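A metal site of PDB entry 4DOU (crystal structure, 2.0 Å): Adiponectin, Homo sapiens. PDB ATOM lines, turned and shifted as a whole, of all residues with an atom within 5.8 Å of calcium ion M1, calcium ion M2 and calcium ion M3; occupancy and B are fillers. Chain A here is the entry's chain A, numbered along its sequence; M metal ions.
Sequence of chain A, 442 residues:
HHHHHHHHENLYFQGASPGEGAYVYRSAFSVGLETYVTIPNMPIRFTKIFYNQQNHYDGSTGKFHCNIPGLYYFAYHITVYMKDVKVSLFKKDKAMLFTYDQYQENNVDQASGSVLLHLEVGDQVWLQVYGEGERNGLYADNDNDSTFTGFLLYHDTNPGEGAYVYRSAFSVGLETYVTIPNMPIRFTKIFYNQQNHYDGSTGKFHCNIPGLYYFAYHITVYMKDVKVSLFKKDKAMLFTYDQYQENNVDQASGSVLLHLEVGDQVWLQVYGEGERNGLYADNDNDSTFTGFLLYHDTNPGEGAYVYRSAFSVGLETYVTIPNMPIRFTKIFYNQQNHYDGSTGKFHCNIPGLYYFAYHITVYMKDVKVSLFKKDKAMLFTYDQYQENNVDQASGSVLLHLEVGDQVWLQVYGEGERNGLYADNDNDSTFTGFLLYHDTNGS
Calcium ion M2 is bound by O of Val 390 (2.3 Å), OD1 of Asp 242 (2.3 Å), OD1 of Asp 250 (2.3 Å), O of Gln 243 (2.4 Å), OD1 of Asn 389 (2.4 Å) and OD1 of Asp 391 (2.5 Å).
O of Asp 391 lies within hydrogen-bond range of N of Val 362 (2.7 Å). ND2 of Asn 389 sits close to ND2 of Asn 248 (3.4 Å). The side-chain amide nitrogen of Asn 107 lies within hydrogen-bond range of the side-chain amide oxygen of Gln 386 (2.9 Å).
Within 4 Å of calcium ion M3: Asp 101, Gln 102, Asp 109, Asn 248, Val 249 and Asp 250. The nearest printed residue that does not touch calcium ion M3 is Tyr 103 (4.7 Å).
Within 4 Å of calcium ion M2: Asp 242, Gln 243, Asp 250, Asn 389, Val 390 and Asp 391. The nearest printed residue that does not touch calcium ion M2 is Tyr 244 (4.6 Å).
Calcium ion M3 is bound by OD2 of Asp 250. Calcium ion M3 is bound by the side-chain carboxylate (OD2) of Asp 109 (2.3 Å). O of Val 249 binds calcium ion M3, at 2.3 Å. Calcium ion M3 is bound by the side-chain carboxylate (OD2) of Asp 101. Calcium ion M3 is bound by OD1 of Asn 248, at 2.5 Å. Calcium ion M3 is bound by O of Gln 102. Calcium ion M3 has six donor atoms within binding distance.
Six residues have an atom within 4 Å of calcium ion M1: Asn 107, Val 108, Asp 109, Asp 383, Gln 384 and Asp 391. The nearest printed residue that does not touch calcium ion M1 is Tyr 385 (4.6 Å).
Calcium ion M1 is bound by the side-chain carboxylate (OD2) of Asp 391 (2.2 Å), the backbone carbonyl oxygen (O) of Val 108 (2.3 Å), the side-chain carboxylate (OD1) of Asp 383 (2.3 Å), the backbone carbonyl oxygen (O) of Gln 384 (2.4 Å), the side-chain carboxylate (OD1) of Asp 109 (2.5 Å) and the side-chain amide oxygen (OD1) of Asn 107 (2.6 Å). Calcium ion M1 has six donor atoms within binding distance.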
ATOM      1  N   ASP A 101      13.819  31.843  17.562  1.00  0.00           N
ATOM      2  CA  ASP A 101      12.787  31.274  16.725  1.00  0.00           C
ATOM      3  C   ASP A 101      13.306  29.932  16.198  1.00  0.00           C
ATOM      4  O   ASP A 101      14.320  29.874  15.514  1.00  0.00           O
ATOM      5  CB  ASP A 101      12.454  32.227  15.568  1.00  0.00           C
ATOM      6  CG  ASP A 101      11.113  31.932  14.897  1.00  0.00           C
ATOM      7  OD1 ASP A 101      10.572  32.840  14.228  1.00  0.00           O
ATOM      8  OD2 ASP A 101      10.616  30.795  15.020  1.00  0.00           O
ATOM      9  N   GLN A 102      12.619  28.849  16.572  1.00  0.00           N
ATOM     10  CA  GLN A 102      13.030  27.507  16.155  1.00  0.00           C
ATOM     11  C   GLN A 102      12.518  27.232  14.745  1.00  0.00           C
ATOM     12  O   GLN A 102      11.466  27.743  14.348  1.00  0.00           O
ATOM     13  CB  GLN A 102      12.494  26.435  17.125  1.00  0.00           C
ATOM     14  CG  GLN A 102      13.416  26.156  18.303  1.00  0.00           C
ATOM     15  CD  GLN A 102      12.836  25.163  19.299  1.00  0.00           C
ATOM     16  OE1 GLN A 102      11.659  25.240  19.664  1.00  0.00           O
ATOM     17  NE2 GLN A 102      13.660  24.233  19.754  1.00  0.00           N
ATOM     18  N   TYR A 103      13.274  26.448  13.985  1.00  0.00           N
ATOM     19  CA  TYR A 103      12.897  26.067  12.636  1.00  0.00           C
ATOM     20  C   TYR A 103      12.492  24.594  12.570  1.00  0.00           C
ATOM     21  O   TYR A 103      13.159  23.724  13.122  1.00  0.00           O
ATOM     22  CB  TYR A 103      14.045  26.289  11.650  1.00  0.00           C
ATOM     23  CG  TYR A 103      13.722  25.797  10.252  1.00  0.00           C
ATOM     24  CD1 TYR A 103      12.881  26.520   9.435  1.00  0.00           C
ATOM     25  CD2 TYR A 103      14.239  24.602   9.781  1.00  0.00           C
ATOM     26  CE1 TYR A 103      12.564  26.070   8.159  1.00  0.00           C
ATOM     27  CE2 TYR A 103      13.925  24.142   8.510  1.00  0.00           C
ATOM     28  CZ  TYR A 103      13.090  24.887   7.705  1.00  0.00           C
ATOM     29  OH  TYR A 103      12.774  24.443   6.442  1.00  0.00           O
ATOM     30  N   ASN A 107       8.993  24.531   7.099  1.00  0.00           N
ATOM     31  CA  ASN A 107       8.237  25.536   7.825  1.00  0.00           C
ATOM     32  C   ASN A 107       8.991  26.853   8.061  1.00  0.00           C
ATOM     33  O   ASN A 107       9.322  27.198   9.191  1.00  0.00           O
ATOM     34  CB  ASN A 107       7.744  24.957   9.141  1.00  0.00           C
ATOM     35  CG  ASN A 107       6.612  25.764   9.727  1.00  0.00           C
ATOM     36  OD1 ASN A 107       6.455  26.933   9.407  1.00  0.00           O
ATOM     37  ND2 ASN A 107       5.816  25.137  10.582  1.00  0.00           N
ATOM     38  N   VAL A 108       9.235  27.592   6.992  1.00  0.00           N
ATOM     39  CA  VAL A 108       9.877  28.892   7.096  1.00  0.00           C
ATOM     40  C   VAL A 108       9.125  29.791   8.076  1.00  0.00           C
ATOM     41  O   VAL A 108       7.887  29.897   8.033  1.00  0.00           O
ATOM     42  CB  VAL A 108       9.975  29.572   5.726  1.00  0.00           C
ATOM     43  CG1 VAL A 108      10.516  30.983   5.844  1.00  0.00           C
ATOM     44  CG2 VAL A 108      10.832  28.708   4.779  1.00  0.00           C
ATOM     45  N   ASP A 109       9.896  30.443   8.952  1.00  0.00           N
ATOM     46  CA  ASP A 109       9.345  31.335   9.972  1.00  0.00           C
ATOM     47  C   ASP A 109       9.790  32.790   9.856  1.00  0.00           C
ATOM     48  O   ASP A 109      10.698  33.133   9.081  1.00  0.00           O
ATOM     49  CB  ASP A 109       9.651  30.808  11.373  1.00  0.00           C
ATOM     50  CG  ASP A 109       8.649  29.773  11.805  1.00  0.00           C
ATOM     51  OD1 ASP A 109       7.589  29.698  11.159  1.00  0.00           O
ATOM     52  OD2 ASP A 109       8.910  29.034  12.785  1.00  0.00           O
ATOM     53  N   GLN A 110       9.146  33.651  10.633  1.00  0.00           N
ATOM     54  CA  GLN A 110       9.495  35.052  10.672  1.00  0.00           C
ATOM     55  C   GLN A 110       9.691  35.486  12.101  1.00  0.00           C
ATOM     56  O   GLN A 110       8.774  35.381  12.906  1.00  0.00           O
ATOM     57  CB  GLN A 110       8.423  35.916  10.006  1.00  0.00           C
ATOM     58  CG  GLN A 110       8.386  35.805   8.500  1.00  0.00           C
ATOM     59  CD  GLN A 110       9.625  36.374   7.839  1.00  0.00           C
ATOM     60  OE1 GLN A 110      10.106  35.857   6.813  1.00  0.00           O
ATOM     61  NE2 GLN A 110      10.139  37.465   8.400  1.00  0.00           N
ATOM     62  N   ASP A 242      -0.808  33.362  17.859  1.00  0.00           N
ATOM     63  CA  ASP A 242       0.297  32.577  17.337  1.00  0.00           C
ATOM     64  C   ASP A 242       0.273  31.194  17.961  1.00  0.00           C
ATOM     65  O   ASP A 242       0.411  31.042  19.179  1.00  0.00           O
ATOM     66  CB  ASP A 242       1.637  33.287  17.588  1.00  0.00           C
ATOM     67  CG  ASP A 242       2.770  32.740  16.718  1.00  0.00           C
ATOM     68  OD1 ASP A 242       2.623  31.614  16.200  1.00  0.00           O
ATOM     69  OD2 ASP A 242       3.808  33.431  16.540  1.00  0.00           O
ATOM     70  N   GLN A 243       0.104  30.181  17.122  1.00  0.00           N
ATOM     71  CA  GLN A 243      -0.071  28.807  17.578  1.00  0.00           C
ATOM     72  C   GLN A 243       1.263  28.148  17.864  1.00  0.00           C
ATOM     73  O   GLN A 243       2.234  28.347  17.131  1.00  0.00           O
ATOM     74  CB  GLN A 243      -0.818  27.979  16.529  1.00  0.00           C
ATOM     75  CG  GLN A 243      -2.224  27.571  16.915  1.00  0.00           C
ATOM     76  CD  GLN A 243      -2.820  26.574  15.928  1.00  0.00           C
ATOM     77  OE1 GLN A 243      -2.806  26.792  14.721  1.00  0.00           O
ATOM     78  NE2 GLN A 243      -3.352  25.473  16.449  1.00  0.00           N
ATOM     79  N   TYR A 244       1.305  27.333  18.911  1.00  0.00           N
ATOM     80  CA  TYR A 244       2.513  26.630  19.277  1.00  0.00           C
ATOM     81  C   TYR A 244       2.438  25.135  19.007  1.00  0.00           C
ATOM     82  O   TYR A 244       1.584  24.439  19.542  1.00  0.00           O
ATOM     83  CB  TYR A 244       2.847  26.846  20.756  1.00  0.00           C
ATOM     84  CG  TYR A 244       4.073  26.070  21.176  1.00  0.00           C
ATOM     85  CD1 TYR A 244       5.343  26.569  20.909  1.00  0.00           C
ATOM     86  CD2 TYR A 244       3.975  24.849  21.823  1.00  0.00           C
ATOM     87  CE1 TYR A 244       6.460  25.885  21.266  1.00  0.00           C
ATOM     88  CE2 TYR A 244       5.103  24.140  22.193  1.00  0.00           C
ATOM     89  CZ  TYR A 244       6.346  24.669  21.912  1.00  0.00           C
ATOM     90  OH  TYR A 244       7.483  24.009  22.253  1.00  0.00           O
ATOM     91  N   GLN A 245       3.353  24.652  18.175  1.00  0.00           N
ATOM     92  CA  GLN A 245       3.513  23.220  18.007  1.00  0.00           C
ATOM     93  C   GLN A 245       4.770  22.795  18.757  1.00  0.00           C
ATOM     94  O   GLN A 245       5.683  23.601  18.968  1.00  0.00           O
ATOM     95  CB  GLN A 245       3.605  22.835  16.543  1.00  0.00           C
ATOM     96  CG  GLN A 245       2.994  21.461  16.249  1.00  0.00           C
ATOM     97  CD  GLN A 245       1.487  21.529  16.061  1.00  0.00           C
ATOM     98  OE1 GLN A 245       0.729  20.884  16.784  1.00  0.00           O
ATOM     99  NE2 GLN A 245       1.049  22.320  15.088  1.00  0.00           N
ATOM    100  N   ASN A 248       8.715  23.835  18.540  1.00  0.00           N
ATOM    101  CA  ASN A 248       8.719  24.923  17.571  1.00  0.00           C
ATOM    102  C   ASN A 248       8.440  26.283  18.200  1.00  0.00           C
ATOM    103  O   ASN A 248       7.367  26.857  17.989  1.00  0.00           O
ATOM    104  CB  ASN A 248       7.728  24.647  16.435  1.00  0.00           C
ATOM    105  CG  ASN A 248       7.963  25.537  15.226  1.00  0.00           C
ATOM    106  OD1 ASN A 248       8.828  26.410  15.234  1.00  0.00           O
ATOM    107  ND2 ASN A 248       7.180  25.324  14.170  1.00  0.00           N
ATOM    108  N   VAL A 249       9.390  26.788  18.976  1.00  0.00           N
ATOM    109  CA  VAL A 249       9.269  28.116  19.539  1.00  0.00           C
ATOM    110  C   VAL A 249       9.052  29.072  18.368  1.00  0.00           C
ATOM    111  O   VAL A 249       9.676  28.955  17.313  1.00  0.00           O
ATOM    112  CB  VAL A 249      10.541  28.548  20.320  1.00  0.00           C
ATOM    113  CG1 VAL A 249      10.497  30.055  20.637  1.00  0.00           C
ATOM    114  CG2 VAL A 249      10.723  27.720  21.603  1.00  0.00           C
ATOM    115  N   ASP A 250       8.123  30.007  18.558  1.00  0.00           N
ATOM    116  CA  ASP A 250       7.773  30.964  17.514  1.00  0.00           C
ATOM    117  C   ASP A 250       7.937  32.394  18.030  1.00  0.00           C
ATOM    118  O   ASP A 250       8.190  32.613  19.231  1.00  0.00           O
ATOM    119  CB  ASP A 250       6.316  30.739  17.046  1.00  0.00           C
ATOM    120  CG  ASP A 250       6.203  29.667  15.957  1.00  0.00           C
ATOM    121  OD1 ASP A 250       5.092  29.110  15.758  1.00  0.00           O
ATOM    122  OD2 ASP A 250       7.207  29.369  15.279  1.00  0.00           O
ATOM    123  N   GLN A 251       7.795  33.348  17.120  1.00  0.00           N
ATOM    124  CA  GLN A 251       7.862  34.763  17.451  1.00  0.00           C
ATOM    125  C   GLN A 251       6.673  35.492  16.865  1.00  0.00           C
ATOM    126  O   GLN A 251       6.365  35.354  15.682  1.00  0.00           O
ATOM    127  CB  GLN A 251       9.155  35.368  16.887  1.00  0.00           C
ATOM    128  CG  GLN A 251      10.411  34.913  17.604  1.00  0.00           C
ATOM    129  CD  GLN A 251      10.535  35.486  18.988  1.00  0.00           C
ATOM    130  OE1 GLN A 251      11.300  34.976  19.816  1.00  0.00           O
ATOM    131  NE2 GLN A 251       9.802  36.584  19.252  1.00  0.00           N
ATOM    132  N   VAL A 362      -0.844  34.305   9.612  1.00  0.00           N
ATOM    133  CA  VAL A 362      -0.604  33.313   8.570  1.00  0.00           C
ATOM    134  C   VAL A 362      -1.450  32.086   8.856  1.00  0.00           C
ATOM    135  O   VAL A 362      -1.191  31.355   9.807  1.00  0.00           O
ATOM    136  CB  VAL A 362       0.879  32.937   8.526  1.00  0.00           C
ATOM    137  CG1 VAL A 362       1.159  31.942   7.375  1.00  0.00           C
ATOM    138  CG2 VAL A 362       1.744  34.202   8.412  1.00  0.00           C
ATOM    139  N   ASP A 383       6.444  33.438   4.766  1.00  0.00           N
ATOM    140  CA  ASP A 383       6.170  32.662   5.973  1.00  0.00           C
ATOM    141  C   ASP A 383       5.318  31.426   5.645  1.00  0.00           C
ATOM    142  O   ASP A 383       4.141  31.523   5.306  1.00  0.00           O
ATOM    143  CB  ASP A 383       5.524  33.552   7.061  1.00  0.00           C
ATOM    144  CG  ASP A 383       5.597  32.924   8.447  1.00  0.00           C
ATOM    145  OD1 ASP A 383       5.918  31.717   8.543  1.00  0.00           O
ATOM    146  OD2 ASP A 383       5.340  33.649   9.446  1.00  0.00           O
ATOM    147  N   GLN A 384       5.945  30.254   5.736  1.00  0.00           N
ATOM    148  CA  GLN A 384       5.241  29.011   5.420  1.00  0.00           C
ATOM    149  C   GLN A 384       4.175  28.668   6.456  1.00  0.00           C
ATOM    150  O   GLN A 384       4.276  29.058   7.619  1.00  0.00           O
ATOM    151  CB  GLN A 384       6.237  27.864   5.275  1.00  0.00           C
ATOM    152  CG  GLN A 384       6.741  27.682   3.864  1.00  0.00           C
ATOM    153  CD  GLN A 384       7.592  26.446   3.705  1.00  0.00           C
ATOM    154  OE1 GLN A 384       8.633  26.313   4.355  1.00  0.00           O
ATOM    155  NE2 GLN A 384       7.161  25.539   2.836  1.00  0.00           N
ATOM    156  N   TYR A 385       3.140  27.958   6.016  1.00  0.00           N
ATOM    157  CA  TYR A 385       2.088  27.538   6.939  1.00  0.00           C
ATOM    158  C   TYR A 385       2.094  26.025   7.079  1.00  0.00           C
ATOM    159  O   TYR A 385       2.129  25.306   6.076  1.00  0.00           O
ATOM    160  CB  TYR A 385       0.704  28.013   6.476  1.00  0.00           C
ATOM    161  CG  TYR A 385      -0.415  27.503   7.368  1.00  0.00           C
ATOM    162  CD1 TYR A 385      -0.715  28.136   8.570  1.00  0.00           C
ATOM    163  CD2 TYR A 385      -1.167  26.378   7.016  1.00  0.00           C
ATOM    164  CE1 TYR A 385      -1.728  27.668   9.393  1.00  0.00           C
ATOM    165  CE2 TYR A 385      -2.187  25.905   7.834  1.00  0.00           C
ATOM    166  CZ  TYR A 385      -2.451  26.556   9.022  1.00  0.00           C
ATOM    167  OH  TYR A 385      -3.459  26.103   9.845  1.00  0.00           O
ATOM    168  N   GLN A 386       2.085  25.562   8.316  1.00  0.00           N
ATOM    169  CA  GLN A 386       1.916  24.136   8.597  1.00  0.00           C
ATOM    170  C   GLN A 386       0.576  23.905   9.300  1.00  0.00           C
ATOM    171  O   GLN A 386       0.177  24.694  10.164  1.00  0.00           O
ATOM    172  CB  GLN A 386       3.081  23.597   9.430  1.00  0.00           C
ATOM    173  CG  GLN A 386       3.087  22.090   9.606  1.00  0.00           C
ATOM    174  CD  GLN A 386       4.410  21.544  10.140  1.00  0.00           C
ATOM    175  OE1 GLN A 386       5.386  22.288  10.298  1.00  0.00           O
ATOM    176  NE2 GLN A 386       4.452  20.240  10.426  1.00  0.00           N
ATOM    177  N   ASN A 389      -0.947  25.235  12.747  1.00  0.00           N
ATOM    178  CA  ASN A 389       0.116  26.129  13.219  1.00  0.00           C
ATOM    179  C   ASN A 389       0.010  27.527  12.634  1.00  0.00           C
ATOM    180  O   ASN A 389       0.817  27.907  11.801  1.00  0.00           O
ATOM    181  CB  ASN A 389       1.504  25.531  12.935  1.00  0.00           C
ATOM    182  CG  ASN A 389       2.612  26.225  13.726  1.00  0.00           C
ATOM    183  OD1 ASN A 389       2.421  27.317  14.275  1.00  0.00           O
ATOM    184  ND2 ASN A 389       3.780  25.595  13.778  1.00  0.00           N
ATOM    185  N   VAL A 390      -0.996  28.284  13.071  1.00  0.00           N
ATOM    186  CA  VAL A 390      -1.081  29.696  12.729  1.00  0.00           C
ATOM    187  C   VAL A 390       0.265  30.338  13.049  1.00  0.00           C
ATOM    188  O   VAL A 390       0.887  30.016  14.073  1.00  0.00           O
ATOM    189  CB  VAL A 390      -2.186  30.406  13.521  1.00  0.00           C
ATOM    190  CG1 VAL A 390      -2.037  31.925  13.434  1.00  0.00           C
ATOM    191  CG2 VAL A 390      -3.562  29.958  13.021  1.00  0.00           C
ATOM    192  N   ASP A 391       0.714  31.236  12.178  1.00  0.00           N
ATOM    193  CA  ASP A 391       1.974  31.964  12.338  1.00  0.00           C
ATOM    194  C   ASP A 391       1.791  33.477  12.243  1.00  0.00           C
ATOM    195  O   ASP A 391       0.765  33.981  11.766  1.00  0.00           O
ATOM    196  CB  ASP A 391       2.993  31.510  11.298  1.00  0.00           C
ATOM    197  CG  ASP A 391       3.799  30.312  11.733  1.00  0.00           C
ATOM    198  OD1 ASP A 391       3.731  29.970  12.926  1.00  0.00           O
ATOM    199  OD2 ASP A 391       4.514  29.725  10.900  1.00  0.00           O
ATOM    200  N   GLN A 392       2.822  34.196  12.678  1.00  0.00           N
ATOM    201  CA  GLN A 392       2.847  35.641  12.614  1.00  0.00           C
ATOM    202  C   GLN A 392       4.093  36.098  11.869  1.00  0.00           C
ATOM    203  O   GLN A 392       5.222  35.787  12.268  1.00  0.00           O
ATOM    204  CB  GLN A 392       2.854  36.248  14.016  1.00  0.00           C
ATOM    205  CG  GLN A 392       1.518  36.157  14.729  1.00  0.00           C
ATOM    206  CD  GLN A 392       0.426  37.027  14.111  1.00  0.00           C
ATOM    207  OE1 GLN A 392       0.695  38.079  13.515  1.00  0.00           O
ATOM    208  NE2 GLN A 392      -0.820  36.588  14.268  1.00  0.00           N
HETATM  209 CA    CA M   1       6.019  29.508   9.273  1.00  0.00          CA
HETATM  210 CA    CA M   2       2.860  29.548  15.183  1.00  0.00          CA
HETATM  211 CA    CA M   3       9.349  28.801  15.025  1.00  0.00          CA
